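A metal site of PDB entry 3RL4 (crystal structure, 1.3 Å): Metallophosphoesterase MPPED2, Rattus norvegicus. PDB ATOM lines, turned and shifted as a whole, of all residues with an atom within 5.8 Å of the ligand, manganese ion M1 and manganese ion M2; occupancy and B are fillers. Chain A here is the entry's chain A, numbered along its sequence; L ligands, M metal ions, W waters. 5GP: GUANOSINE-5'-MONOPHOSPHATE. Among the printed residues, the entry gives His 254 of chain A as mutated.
A ring nitrogen (NE2) of His 120 is in hydrogen-bond range of an oxygen (O3P) of the ligand (2.6 Å). OE1 of Glu 257 is in hydrogen-bond range of O3' of the ligand. O3' of the ligand is in hydrogen-bond range of N of His 256 (2.9 Å). O of His 254 lies close to O3' of the ligand, at 3.4 Å. A nitrogen (N2) of the ligand lies within hydrogen-bond range of the side-chain carboxylate of Glu 228.
The side-chain carboxylate (OD1) of Asp 88 is in hydrogen-bond range of the backbone NH (N) of His 120, at 2.9 Å. O of Val 232 is in hydrogen-bond range of NH2 of Arg 194 (2.8 Å). O of Thr 276 is in hydrogen-bond range of ND1 of His 256. OD2 of Asp 67 is in hydrogen-bond range of N of His 254 (2.9 Å). O of Gly 87 sits at hydrogen-bond distance from N of Asp 67 (2.8 Å). N of Val 225 lies within hydrogen-bond range of O of Gln 230 (2.9 Å).
Merely in contact with the ligand: Phe 185 (3.3 Å), Phe 279 (3.6 Å), Val 232 (3.6 Å), Val 277 (3.7 Å), Ile 255 (3.8 Å) and Val 225 (3.9 Å). Hydrophobic or aromatic side chains within 4 Å of the ligand: His 69, His 120, Phe 185, Val 225, Val 232, His 254, Ile 255, His 256, Val 277 and Phe 279. Within 4 Å of the ligand: His 69, Asp 88, Asn 119, His 120, Phe 185, Val 225, Glu 228, Val 232, His 254, Ile 255, His 256, Glu 257, Val 277 and Phe 279. The nearest printed residue that does not touch the ligand is Asp 67 (4.1 Å).
Of the 24 residues printed, 4 come within 4 Å of manganese ion M1. The nearest printed residue that does not touch manganese ion M1 is His 254 (4.3 Å).
Of the 24 residues printed, 5 come within 4 Å of manganese ion M2. The nearest printed residue that does not touch manganese ion M2 is His 120 (4.5 Å).
Manganese ion M1 is bound by the side-chain carboxylate of Asp 67 (2.1 Å), water W4 (2.1 Å), an oxygen (O2P) of the ligand (2.1 Å), a ring nitrogen (NE2) of His 69 (2.2 Å), a ring nitrogen (NE2) of His 256 (2.2 Å) and the side-chain carboxylate of Asp 88 (2.2 Å). Manganese ion M1 has six donor atoms within binding distance.
Water W4 is bound to manganese ion M2, at 1.9 Å. Manganese ion M2 is bound by OD1 of Asn 119. Manganese ion M2 is bound by O1P of the ligand, at 2.2 Å. Manganese ion M2 is bound by NE2 of His 215, at 2.2 Å. OD2 of Asp 88 is bound to manganese ion M2 (2.3 Å). A ring nitrogen (ND1) of His 254 binds manganese ion M2. Manganese ion M2 has six donor atoms within binding distance.
Water W4 lies within hydrogen-bond range of the backbone carbonyl oxygen of His 254 (2.8 Å) and an oxygen (O5') of the ligand (3.2 Å). Water W3 lies within hydrogen-bond range of an oxygen (O6) of the ligand (2.8 Å), the backbone carbonyl oxygen (O) of Trp 184 (3.2 Å) and the guanidinium group (NH2) of Arg 194 (3.2 Å). Water W5 lies within hydrogen-bond range of an oxygen (O6) of the ligand, the backbone carbonyl oxygen of Pro 183 and a ring nitrogen (NE2) of His 254.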
ATOM      1  N   ASP A  67     -21.231  26.150 -29.522  1.00  0.00           N
ATOM      2  CA  ASP A  67     -19.767  26.132 -29.562  1.00  0.00           C
ATOM      3  C   ASP A  67     -19.297  25.644 -30.925  1.00  0.00           C
ATOM      4  O   ASP A  67     -18.404  24.792 -31.040  1.00  0.00           O
ATOM      5  CB  ASP A  67     -19.218  25.255 -28.430  1.00  0.00           C
ATOM      6  CG  ASP A  67     -19.537  25.855 -27.082  1.00  0.00           C
ATOM      7  OD1 ASP A  67     -18.753  26.704 -26.628  1.00  0.00           O
ATOM      8  OD2 ASP A  67     -20.594  25.515 -26.513  1.00  0.00           O
ATOM      9  N   HIS A  69     -17.969  27.856 -33.004  1.00  0.00           N
ATOM     10  CA  HIS A  69     -16.676  28.558 -33.069  1.00  0.00           C
ATOM     11  C   HIS A  69     -16.243  28.859 -34.507  1.00  0.00           C
ATOM     12  O   HIS A  69     -15.058  28.766 -34.838  1.00  0.00           O
ATOM     13  CB  HIS A  69     -15.598  27.803 -32.266  1.00  0.00           C
ATOM     14  CG  HIS A  69     -15.746  27.925 -30.776  1.00  0.00           C
ATOM     15  ND1 HIS A  69     -15.411  29.076 -30.088  1.00  0.00           N
ATOM     16  CD2 HIS A  69     -16.252  27.072 -29.843  1.00  0.00           C
ATOM     17  CE1 HIS A  69     -15.652  28.909 -28.807  1.00  0.00           C
ATOM     18  NE2 HIS A  69     -16.166  27.705 -28.628  1.00  0.00           N
ATOM     19  N   GLY A  87     -24.489  29.293 -28.069  1.00  0.00           N
ATOM     20  CA  GLY A  87     -23.467  30.352 -27.946  1.00  0.00           C
ATOM     21  C   GLY A  87     -22.084  29.902 -28.383  1.00  0.00           C
ATOM     22  O   GLY A  87     -21.844  28.736 -28.732  1.00  0.00           O
ATOM     23  N   ASP A  88     -21.131  30.834 -28.335  1.00  0.00           N
ATOM     24  CA  ASP A  88     -19.794  30.605 -28.923  1.00  0.00           C
ATOM     25  C   ASP A  88     -19.945  30.206 -30.400  1.00  0.00           C
ATOM     26  O   ASP A  88     -19.369  29.199 -30.867  1.00  0.00           O
ATOM     27  CB  ASP A  88     -18.978  29.563 -28.149  1.00  0.00           C
ATOM     28  CG  ASP A  88     -18.299  30.137 -26.900  1.00  0.00           C
ATOM     29  OD1 ASP A  88     -18.457  31.350 -26.612  1.00  0.00           O
ATOM     30  OD2 ASP A  88     -17.626  29.318 -26.203  1.00  0.00           O
ATOM     31  N   GLY A 118     -22.292  33.363 -26.343  1.00  0.00           N
ATOM     32  CA  GLY A 118     -21.408  32.855 -25.313  1.00  0.00           C
ATOM     33  C   GLY A 118     -20.246  33.807 -25.047  1.00  0.00           C
ATOM     34  O   GLY A 118     -20.228  34.963 -25.514  1.00  0.00           O
ATOM     35  N   ASN A 119     -19.251  33.291 -24.342  1.00  0.00           N
ATOM     36  CA  ASN A 119     -18.147  34.134 -23.894  1.00  0.00           C
ATOM     37  C   ASN A 119     -17.248  34.627 -25.020  1.00  0.00           C
ATOM     38  O   ASN A 119     -16.515  35.619 -24.853  1.00  0.00           O
ATOM     39  CB  ASN A 119     -17.349  33.463 -22.762  1.00  0.00           C
ATOM     40  CG  ASN A 119     -16.875  32.110 -23.116  1.00  0.00           C
ATOM     41  OD1 ASN A 119     -17.683  31.228 -23.438  1.00  0.00           O
ATOM     42  ND2 ASN A 119     -15.580  31.890 -23.066  1.00  0.00           N
ATOM     43  N   HIS A 120     -17.259  33.932 -26.167  1.00  0.00           N
ATOM     44  CA  HIS A 120     -16.461  34.411 -27.304  1.00  0.00           C
ATOM     45  C   HIS A 120     -17.088  35.546 -28.083  1.00  0.00           C
ATOM     46  O   HIS A 120     -16.414  36.146 -28.922  1.00  0.00           O
ATOM     47  CB  HIS A 120     -16.098  33.258 -28.239  1.00  0.00           C
ATOM     48  CG  HIS A 120     -15.037  32.371 -27.689  1.00  0.00           C
ATOM     49  ND1 HIS A 120     -13.747  32.351 -28.201  1.00  0.00           N
ATOM     50  CD2 HIS A 120     -15.029  31.524 -26.633  1.00  0.00           C
ATOM     51  CE1 HIS A 120     -13.018  31.485 -27.522  1.00  0.00           C
ATOM     52  NE2 HIS A 120     -13.768  30.973 -26.562  1.00  0.00           N
ATOM     53  N   PRO A 183     -19.967  31.633 -15.098  1.00  0.00           N
ATOM     54  CA  PRO A 183     -18.994  31.914 -14.039  1.00  0.00           C
ATOM     55  C   PRO A 183     -17.678  32.417 -14.603  1.00  0.00           C
ATOM     56  O   PRO A 183     -17.157  31.834 -15.564  1.00  0.00           O
ATOM     57  CB  PRO A 183     -18.794  30.542 -13.388  1.00  0.00           C
ATOM     58  CG  PRO A 183     -20.099  29.827 -13.592  1.00  0.00           C
ATOM     59  CD  PRO A 183     -20.553  30.277 -14.966  1.00  0.00           C
ATOM     60  N   TRP A 184     -17.134  33.450 -13.974  1.00  0.00           N
ATOM     61  CA  TRP A 184     -15.901  34.108 -14.410  1.00  0.00           C
ATOM     62  C   TRP A 184     -14.786  33.084 -14.609  1.00  0.00           C
ATOM     63  O   TRP A 184     -14.529  32.229 -13.757  1.00  0.00           O
ATOM     64  CB  TRP A 184     -15.486  35.174 -13.393  1.00  0.00           C
ATOM     65  CG  TRP A 184     -14.634  36.331 -13.945  1.00  0.00           C
ATOM     66  CD1 TRP A 184     -15.087  37.560 -14.327  1.00  0.00           C
ATOM     67  CD2 TRP A 184     -13.216  36.354 -14.138  1.00  0.00           C
ATOM     68  NE1 TRP A 184     -14.038  38.348 -14.759  1.00  0.00           N
ATOM     69  CE2 TRP A 184     -12.883  37.629 -14.657  1.00  0.00           C
ATOM     70  CE3 TRP A 184     -12.186  35.420 -13.944  1.00  0.00           C
ATOM     71  CZ2 TRP A 184     -11.567  38.001 -14.970  1.00  0.00           C
ATOM     72  CZ3 TRP A 184     -10.874  35.799 -14.254  1.00  0.00           C
ATOM     73  CH2 TRP A 184     -10.589  37.069 -14.761  1.00  0.00           C
ATOM     74  N   PHE A 185     -14.155  33.176 -15.761  1.00  0.00           N
ATOM     75  CA  PHE A 185     -13.028  32.325 -16.069  1.00  0.00           C
ATOM     76  C   PHE A 185     -11.803  33.183 -16.470  1.00  0.00           C
ATOM     77  O   PHE A 185     -10.750  33.091 -15.830  1.00  0.00           O
ATOM     78  CB  PHE A 185     -13.447  31.319 -17.145  1.00  0.00           C
ATOM     79  CG  PHE A 185     -12.348  30.396 -17.571  1.00  0.00           C
ATOM     80  CD1 PHE A 185     -11.661  29.619 -16.645  1.00  0.00           C
ATOM     81  CD2 PHE A 185     -11.998  30.295 -18.913  1.00  0.00           C
ATOM     82  CE1 PHE A 185     -10.639  28.753 -17.048  1.00  0.00           C
ATOM     83  CE2 PHE A 185     -10.982  29.434 -19.337  1.00  0.00           C
ATOM     84  CZ  PHE A 185     -10.300  28.661 -18.394  1.00  0.00           C
ATOM     85  N   ASN A 186     -11.979  34.063 -17.447  1.00  0.00           N
ATOM     86  CA  ASN A 186     -10.849  34.864 -17.978  1.00  0.00           C
ATOM     87  C   ASN A 186     -11.248  36.288 -18.349  1.00  0.00           C
ATOM     88  O   ASN A 186     -10.480  36.996 -18.981  1.00  0.00           O
ATOM     89  CB  ASN A 186     -10.223  34.180 -19.198  1.00  0.00           C
ATOM     90  CG  ASN A 186     -11.260  33.783 -20.234  1.00  0.00           C
ATOM     91  OD1 ASN A 186     -12.405  34.269 -20.207  1.00  0.00           O
ATOM     92  ND2 ASN A 186     -10.882  32.910 -21.153  1.00  0.00           N
ATOM     93  N   ARG A 194     -19.133  34.145  -9.368  1.00  0.00           N
ATOM     94  CA  ARG A 194     -20.088  33.247  -8.758  1.00  0.00           C
ATOM     95  C   ARG A 194     -20.853  33.915  -7.620  1.00  0.00           C
ATOM     96  O   ARG A 194     -20.359  34.856  -6.981  1.00  0.00           O
ATOM     97  CB  ARG A 194     -19.383  31.968  -8.280  1.00  0.00           C
ATOM     98  CG  ARG A 194     -18.889  31.096  -9.426  1.00  0.00           C
ATOM     99  CD  ARG A 194     -18.090  29.859  -8.957  1.00  0.00           C
ATOM    100  NE  ARG A 194     -17.480  29.166 -10.088  1.00  0.00           N
ATOM    101  CZ  ARG A 194     -18.102  28.253 -10.844  1.00  0.00           C
ATOM    102  NH1 ARG A 194     -19.365  27.903 -10.597  1.00  0.00           N
ATOM    103  NH2 ARG A 194     -17.453  27.716 -11.865  1.00  0.00           N
ATOM    104  N   HIS A 215     -25.388  29.683 -21.838  1.00  0.00           N
ATOM    105  CA  HIS A 215     -24.194  29.278 -22.533  1.00  0.00           C
ATOM    106  C   HIS A 215     -23.509  28.119 -21.824  1.00  0.00           C
ATOM    107  O   HIS A 215     -23.007  27.193 -22.460  1.00  0.00           O
ATOM    108  CB  HIS A 215     -23.213  30.411 -22.782  1.00  0.00           C
ATOM    109  CG  HIS A 215     -21.957  29.948 -23.462  1.00  0.00           C
ATOM    110  ND1 HIS A 215     -21.973  29.229 -24.643  1.00  0.00           N
ATOM    111  CD2 HIS A 215     -20.646  30.072 -23.118  1.00  0.00           C
ATOM    112  CE1 HIS A 215     -20.735  28.912 -24.979  1.00  0.00           C
ATOM    113  NE2 HIS A 215     -19.905  29.399 -24.073  1.00  0.00           N
ATOM    114  N   VAL A 225     -14.481  19.329 -15.933  1.00  0.00           N
ATOM    115  CA  VAL A 225     -13.322  19.768 -16.717  1.00  0.00           C
ATOM    116  C   VAL A 225     -12.134  18.871 -16.353  1.00  0.00           C
ATOM    117  O   VAL A 225     -11.552  19.040 -15.272  1.00  0.00           O
ATOM    118  CB  VAL A 225     -12.972  21.256 -16.489  1.00  0.00           C
ATOM    119  CG1 VAL A 225     -11.751  21.688 -17.321  1.00  0.00           C
ATOM    120  CG2 VAL A 225     -14.163  22.134 -16.839  1.00  0.00           C
ATOM    121  N   GLU A 228      -8.544  20.365 -15.020  1.00  0.00           N
ATOM    122  CA  GLU A 228      -8.477  20.887 -13.654  1.00  0.00           C
ATOM    123  C   GLU A 228      -9.009  19.912 -12.613  1.00  0.00           C
ATOM    124  O   GLU A 228      -8.889  20.171 -11.416  1.00  0.00           O
ATOM    125  CB  GLU A 228      -9.200  22.231 -13.538  1.00  0.00           C
ATOM    126  CG  GLU A 228      -8.403  23.437 -14.047  1.00  0.00           C
ATOM    127  CD  GLU A 228      -8.428  23.556 -15.552  1.00  0.00           C
ATOM    128  OE1 GLU A 228      -9.324  22.970 -16.195  1.00  0.00           O
ATOM    129  OE2 GLU A 228      -7.544  24.247 -16.110  1.00  0.00           O
ATOM    130  N   GLN A 230     -12.128  19.404 -11.901  1.00  0.00           N
ATOM    131  CA  GLN A 230     -13.102  20.204 -11.169  1.00  0.00           C
ATOM    132  C   GLN A 230     -14.430  20.241 -11.914  1.00  0.00           C
ATOM    133  O   GLN A 230     -14.474  20.219 -13.141  1.00  0.00           O
ATOM    134  CB  GLN A 230     -12.603  21.650 -10.993  1.00  0.00           C
ATOM    135  CG  GLN A 230     -11.447  21.813 -10.026  1.00  0.00           C
ATOM    136  CD  GLN A 230     -11.153  23.254  -9.643  1.00  0.00           C
ATOM    137  OE1 GLN A 230     -11.652  24.199 -10.270  1.00  0.00           O
ATOM    138  NE2 GLN A 230     -10.330  23.440  -8.608  1.00  0.00           N
ATOM    139  N   VAL A 232     -17.438  22.750 -12.841  1.00  0.00           N
ATOM    140  CA  VAL A 232     -17.407  24.199 -13.038  1.00  0.00           C
ATOM    141  C   VAL A 232     -18.792  24.783 -13.316  1.00  0.00           C
ATOM    142  O   VAL A 232     -18.894  25.981 -13.552  1.00  0.00           O
ATOM    143  CB  VAL A 232     -16.416  24.636 -14.147  1.00  0.00           C
ATOM    144  CG1 VAL A 232     -14.980  24.111 -13.856  1.00  0.00           C
ATOM    145  CG2 VAL A 232     -16.893  24.148 -15.513  1.00  0.00           C
ATOM    146  N   HIS A 254     -20.486  25.347 -23.648  1.00  0.00           N
ATOM    147  CA  HIS A 254     -19.367  26.000 -22.936  1.00  0.00           C
ATOM    148  C   HIS A 254     -18.262  25.049 -22.522  1.00  0.00           C
ATOM    149  O   HIS A 254     -17.084  25.316 -22.793  1.00  0.00           O
ATOM    150  CB  HIS A 254     -19.887  26.849 -21.770  1.00  0.00           C
ATOM    151  CG  HIS A 254     -18.841  27.688 -21.102  1.00  0.00           C
ATOM    152  ND1 HIS A 254     -18.004  28.553 -21.785  1.00  0.00           N
ATOM    153  CD2 HIS A 254     -18.523  27.799 -19.793  1.00  0.00           C
ATOM    154  CE1 HIS A 254     -17.239  29.190 -20.915  1.00  0.00           C
ATOM    155  NE2 HIS A 254     -17.532  28.744 -19.699  1.00  0.00           N
ATOM    156  N   ILE A 255     -18.652  24.005 -21.793  1.00  0.00           N
ATOM    157  CA  ILE A 255     -17.696  22.965 -21.416  1.00  0.00           C
ATOM    158  C   ILE A 255     -17.727  21.900 -22.489  1.00  0.00           C
ATOM    159  O   ILE A 255     -18.581  20.990 -22.462  1.00  0.00           O
ATOM    160  CB  ILE A 255     -17.998  22.419 -20.005  1.00  0.00           C
ATOM    161  CG1 ILE A 255     -18.043  23.570 -18.974  1.00  0.00           C
ATOM    162  CG2 ILE A 255     -16.987  21.321 -19.622  1.00  0.00           C
ATOM    163  CD1 ILE A 255     -16.842  24.529 -18.990  1.00  0.00           C
ATOM    164  N   HIS A 256     -16.834  22.058 -23.463  1.00  0.00           N
ATOM    165  CA  HIS A 256     -16.914  21.237 -24.685  1.00  0.00           C
ATOM    166  C   HIS A 256     -16.854  19.751 -24.369  1.00  0.00           C
ATOM    167  O   HIS A 256     -17.556  18.935 -24.999  1.00  0.00           O
ATOM    168  CB  HIS A 256     -15.782  21.611 -25.638  1.00  0.00           C
ATOM    169  CG  HIS A 256     -15.827  23.015 -26.168  1.00  0.00           C
ATOM    170  ND1 HIS A 256     -14.893  23.460 -27.081  1.00  0.00           N
ATOM    171  CD2 HIS A 256     -16.641  24.079 -25.909  1.00  0.00           C
ATOM    172  CE1 HIS A 256     -15.132  24.731 -27.375  1.00  0.00           C
ATOM    173  NE2 HIS A 256     -16.181  25.129 -26.678  1.00  0.00           N
ATOM    174  N   GLU A 257     -16.044  19.409 -23.369  1.00  0.00           N
ATOM    175  CA  GLU A 257     -15.787  18.036 -22.926  1.00  0.00           C
ATOM    176  C   GLU A 257     -17.057  17.360 -22.438  1.00  0.00           C
ATOM    177  O   GLU A 257     -17.135  16.133 -22.392  1.00  0.00           O
ATOM    178  CB  GLU A 257     -14.767  18.002 -21.780  1.00  0.00           C
ATOM    179  CG  GLU A 257     -13.413  18.677 -22.018  1.00  0.00           C
ATOM    180  CD  GLU A 257     -13.420  20.109 -21.542  1.00  0.00           C
ATOM    181  OE1 GLU A 257     -14.186  20.901 -22.092  1.00  0.00           O
ATOM    182  OE2 GLU A 257     -12.621  20.477 -20.651  1.00  0.00           O
ATOM    183  N   THR A 276     -15.013  19.879 -29.854  1.00  0.00           N
ATOM    184  CA  THR A 276     -14.343  19.219 -28.737  1.00  0.00           C
ATOM    185  C   THR A 276     -13.452  20.247 -27.998  1.00  0.00           C
ATOM    186  O   THR A 276     -13.347  21.419 -28.393  1.00  0.00           O
ATOM    187  CB  THR A 276     -13.426  18.124 -29.277  1.00  0.00           C
ATOM    188  OG1 THR A 276     -12.445  18.742 -30.112  1.00  0.00           O
ATOM    189  CG2 THR A 276     -14.228  17.077 -30.060  1.00  0.00           C
ATOM    190  N   VAL A 277     -12.811  19.817 -26.918  1.00  0.00           N
ATOM    191  CA  VAL A 277     -11.908  20.699 -26.190  1.00  0.00           C
ATOM    192  C   VAL A 277     -10.738  21.228 -27.057  1.00  0.00           C
ATOM    193  O   VAL A 277     -10.156  22.278 -26.761  1.00  0.00           O
ATOM    194  CB  VAL A 277     -11.427  20.054 -24.864  1.00  0.00           C
ATOM    195  CG1 VAL A 277     -10.482  18.896 -25.137  1.00  0.00           C
ATOM    196  CG2 VAL A 277     -10.805  21.110 -23.905  1.00  0.00           C
ATOM    197  N   PHE A 279     -11.275  22.107 -30.140  1.00  0.00           N
ATOM    198  CA  PHE A 279     -11.943  22.976 -31.118  1.00  0.00           C
ATOM    199  C   PHE A 279     -12.169  22.297 -32.490  1.00  0.00           C
ATOM    200  O   PHE A 279     -12.181  22.966 -33.532  1.00  0.00           O
ATOM    201  CB  PHE A 279     -11.236  24.352 -31.229  1.00  0.00           C
ATOM    202  CG  PHE A 279     -11.542  25.303 -30.088  1.00  0.00           C
ATOM    203  CD1 PHE A 279     -11.039  25.074 -28.800  1.00  0.00           C
ATOM    204  CD2 PHE A 279     -12.332  26.430 -30.288  1.00  0.00           C
ATOM    205  CE1 PHE A 279     -11.328  25.962 -27.748  1.00  0.00           C
ATOM    206  CE2 PHE A 279     -12.611  27.315 -29.244  1.00  0.00           C
ATOM    207  CZ  PHE A 279     -12.121  27.079 -27.984  1.00  0.00           C
HETATM  208  P   5GP L   1     -14.522  28.493 -24.435  1.00  0.00           P
HETATM  209  O1P 5GP L   1     -15.544  29.297 -23.742  1.00  0.00           O
HETATM  210  O2P 5GP L   1     -14.915  28.049 -25.941  1.00  0.00           O
HETATM  211  O3P 5GP L   1     -13.195  29.311 -24.586  1.00  0.00           O
HETATM  212  O5' 5GP L   1     -14.204  27.167 -23.597  1.00  0.00           O
HETATM  213  C5' 5GP L   1     -13.228  26.207 -24.067  1.00  0.00           C
HETATM  214  C4' 5GP L   1     -12.797  25.282 -22.946  1.00  0.00           C
HETATM  215  O4' 5GP L   1     -12.295  26.108 -21.884  1.00  0.00           O
HETATM  216  C3' 5GP L   1     -13.908  24.495 -22.253  1.00  0.00           C
HETATM  217  O3' 5GP L   1     -14.283  23.340 -23.037  1.00  0.00           O
HETATM  218  C2' 5GP L   1     -13.221  24.126 -20.943  1.00  0.00           C
HETATM  219  O2' 5GP L   1     -12.256  23.081 -21.142  1.00  0.00           O
HETATM  220  C1' 5GP L   1     -12.453  25.429 -20.636  1.00  0.00           C
HETATM  221  N9  5GP L   1     -13.269  26.269 -19.710  1.00  0.00           N
HETATM  222  C8  5GP L   1     -14.289  27.105 -20.002  1.00  0.00           C
HETATM  223  N7  5GP L   1     -14.741  27.645 -18.879  1.00  0.00           N
HETATM  224  C5  5GP L   1     -14.036  27.155 -17.863  1.00  0.00           C
HETATM  225  C6  5GP L   1     -14.067  27.341 -16.487  1.00  0.00           C
HETATM  226  O6  5GP L   1     -14.866  28.104 -15.928  1.00  0.00           O
HETATM  227  N1  5GP L   1     -13.149  26.657 -15.713  1.00  0.00           N
HETATM  228  C2  5GP L   1     -12.229  25.780 -16.303  1.00  0.00           C
HETATM  229  N2  5GP L   1     -11.361  25.140 -15.526  1.00  0.00           N
HETATM  230  N3  5GP L   1     -12.210  25.615 -17.631  1.00  0.00           N
HETATM  231  C4  5GP L   1     -13.096  26.280 -18.405  1.00  0.00           C
HETATM  232 MN    MN M   1     -16.769  27.277 -26.594  1.00  0.00          MN
HETATM  233 MN    MN M   2     -17.702  29.178 -23.951  1.00  0.00          MN
HETATM  234  O   HOH W   1     -12.224  27.104 -13.140  1.00  0.00           O
HETATM  235  O   HOH W   2      -9.659  22.672 -20.392  1.00  0.00           O
HETATM  236  O   HOH W   3     -14.939  29.085 -13.339  1.00  0.00           O
HETATM  237  O   HOH W   4     -17.195  27.419 -24.563  1.00  0.00           O
HETATM  238  O   HOH W   5     -17.355  29.063 -16.692  1.00  0.00           O
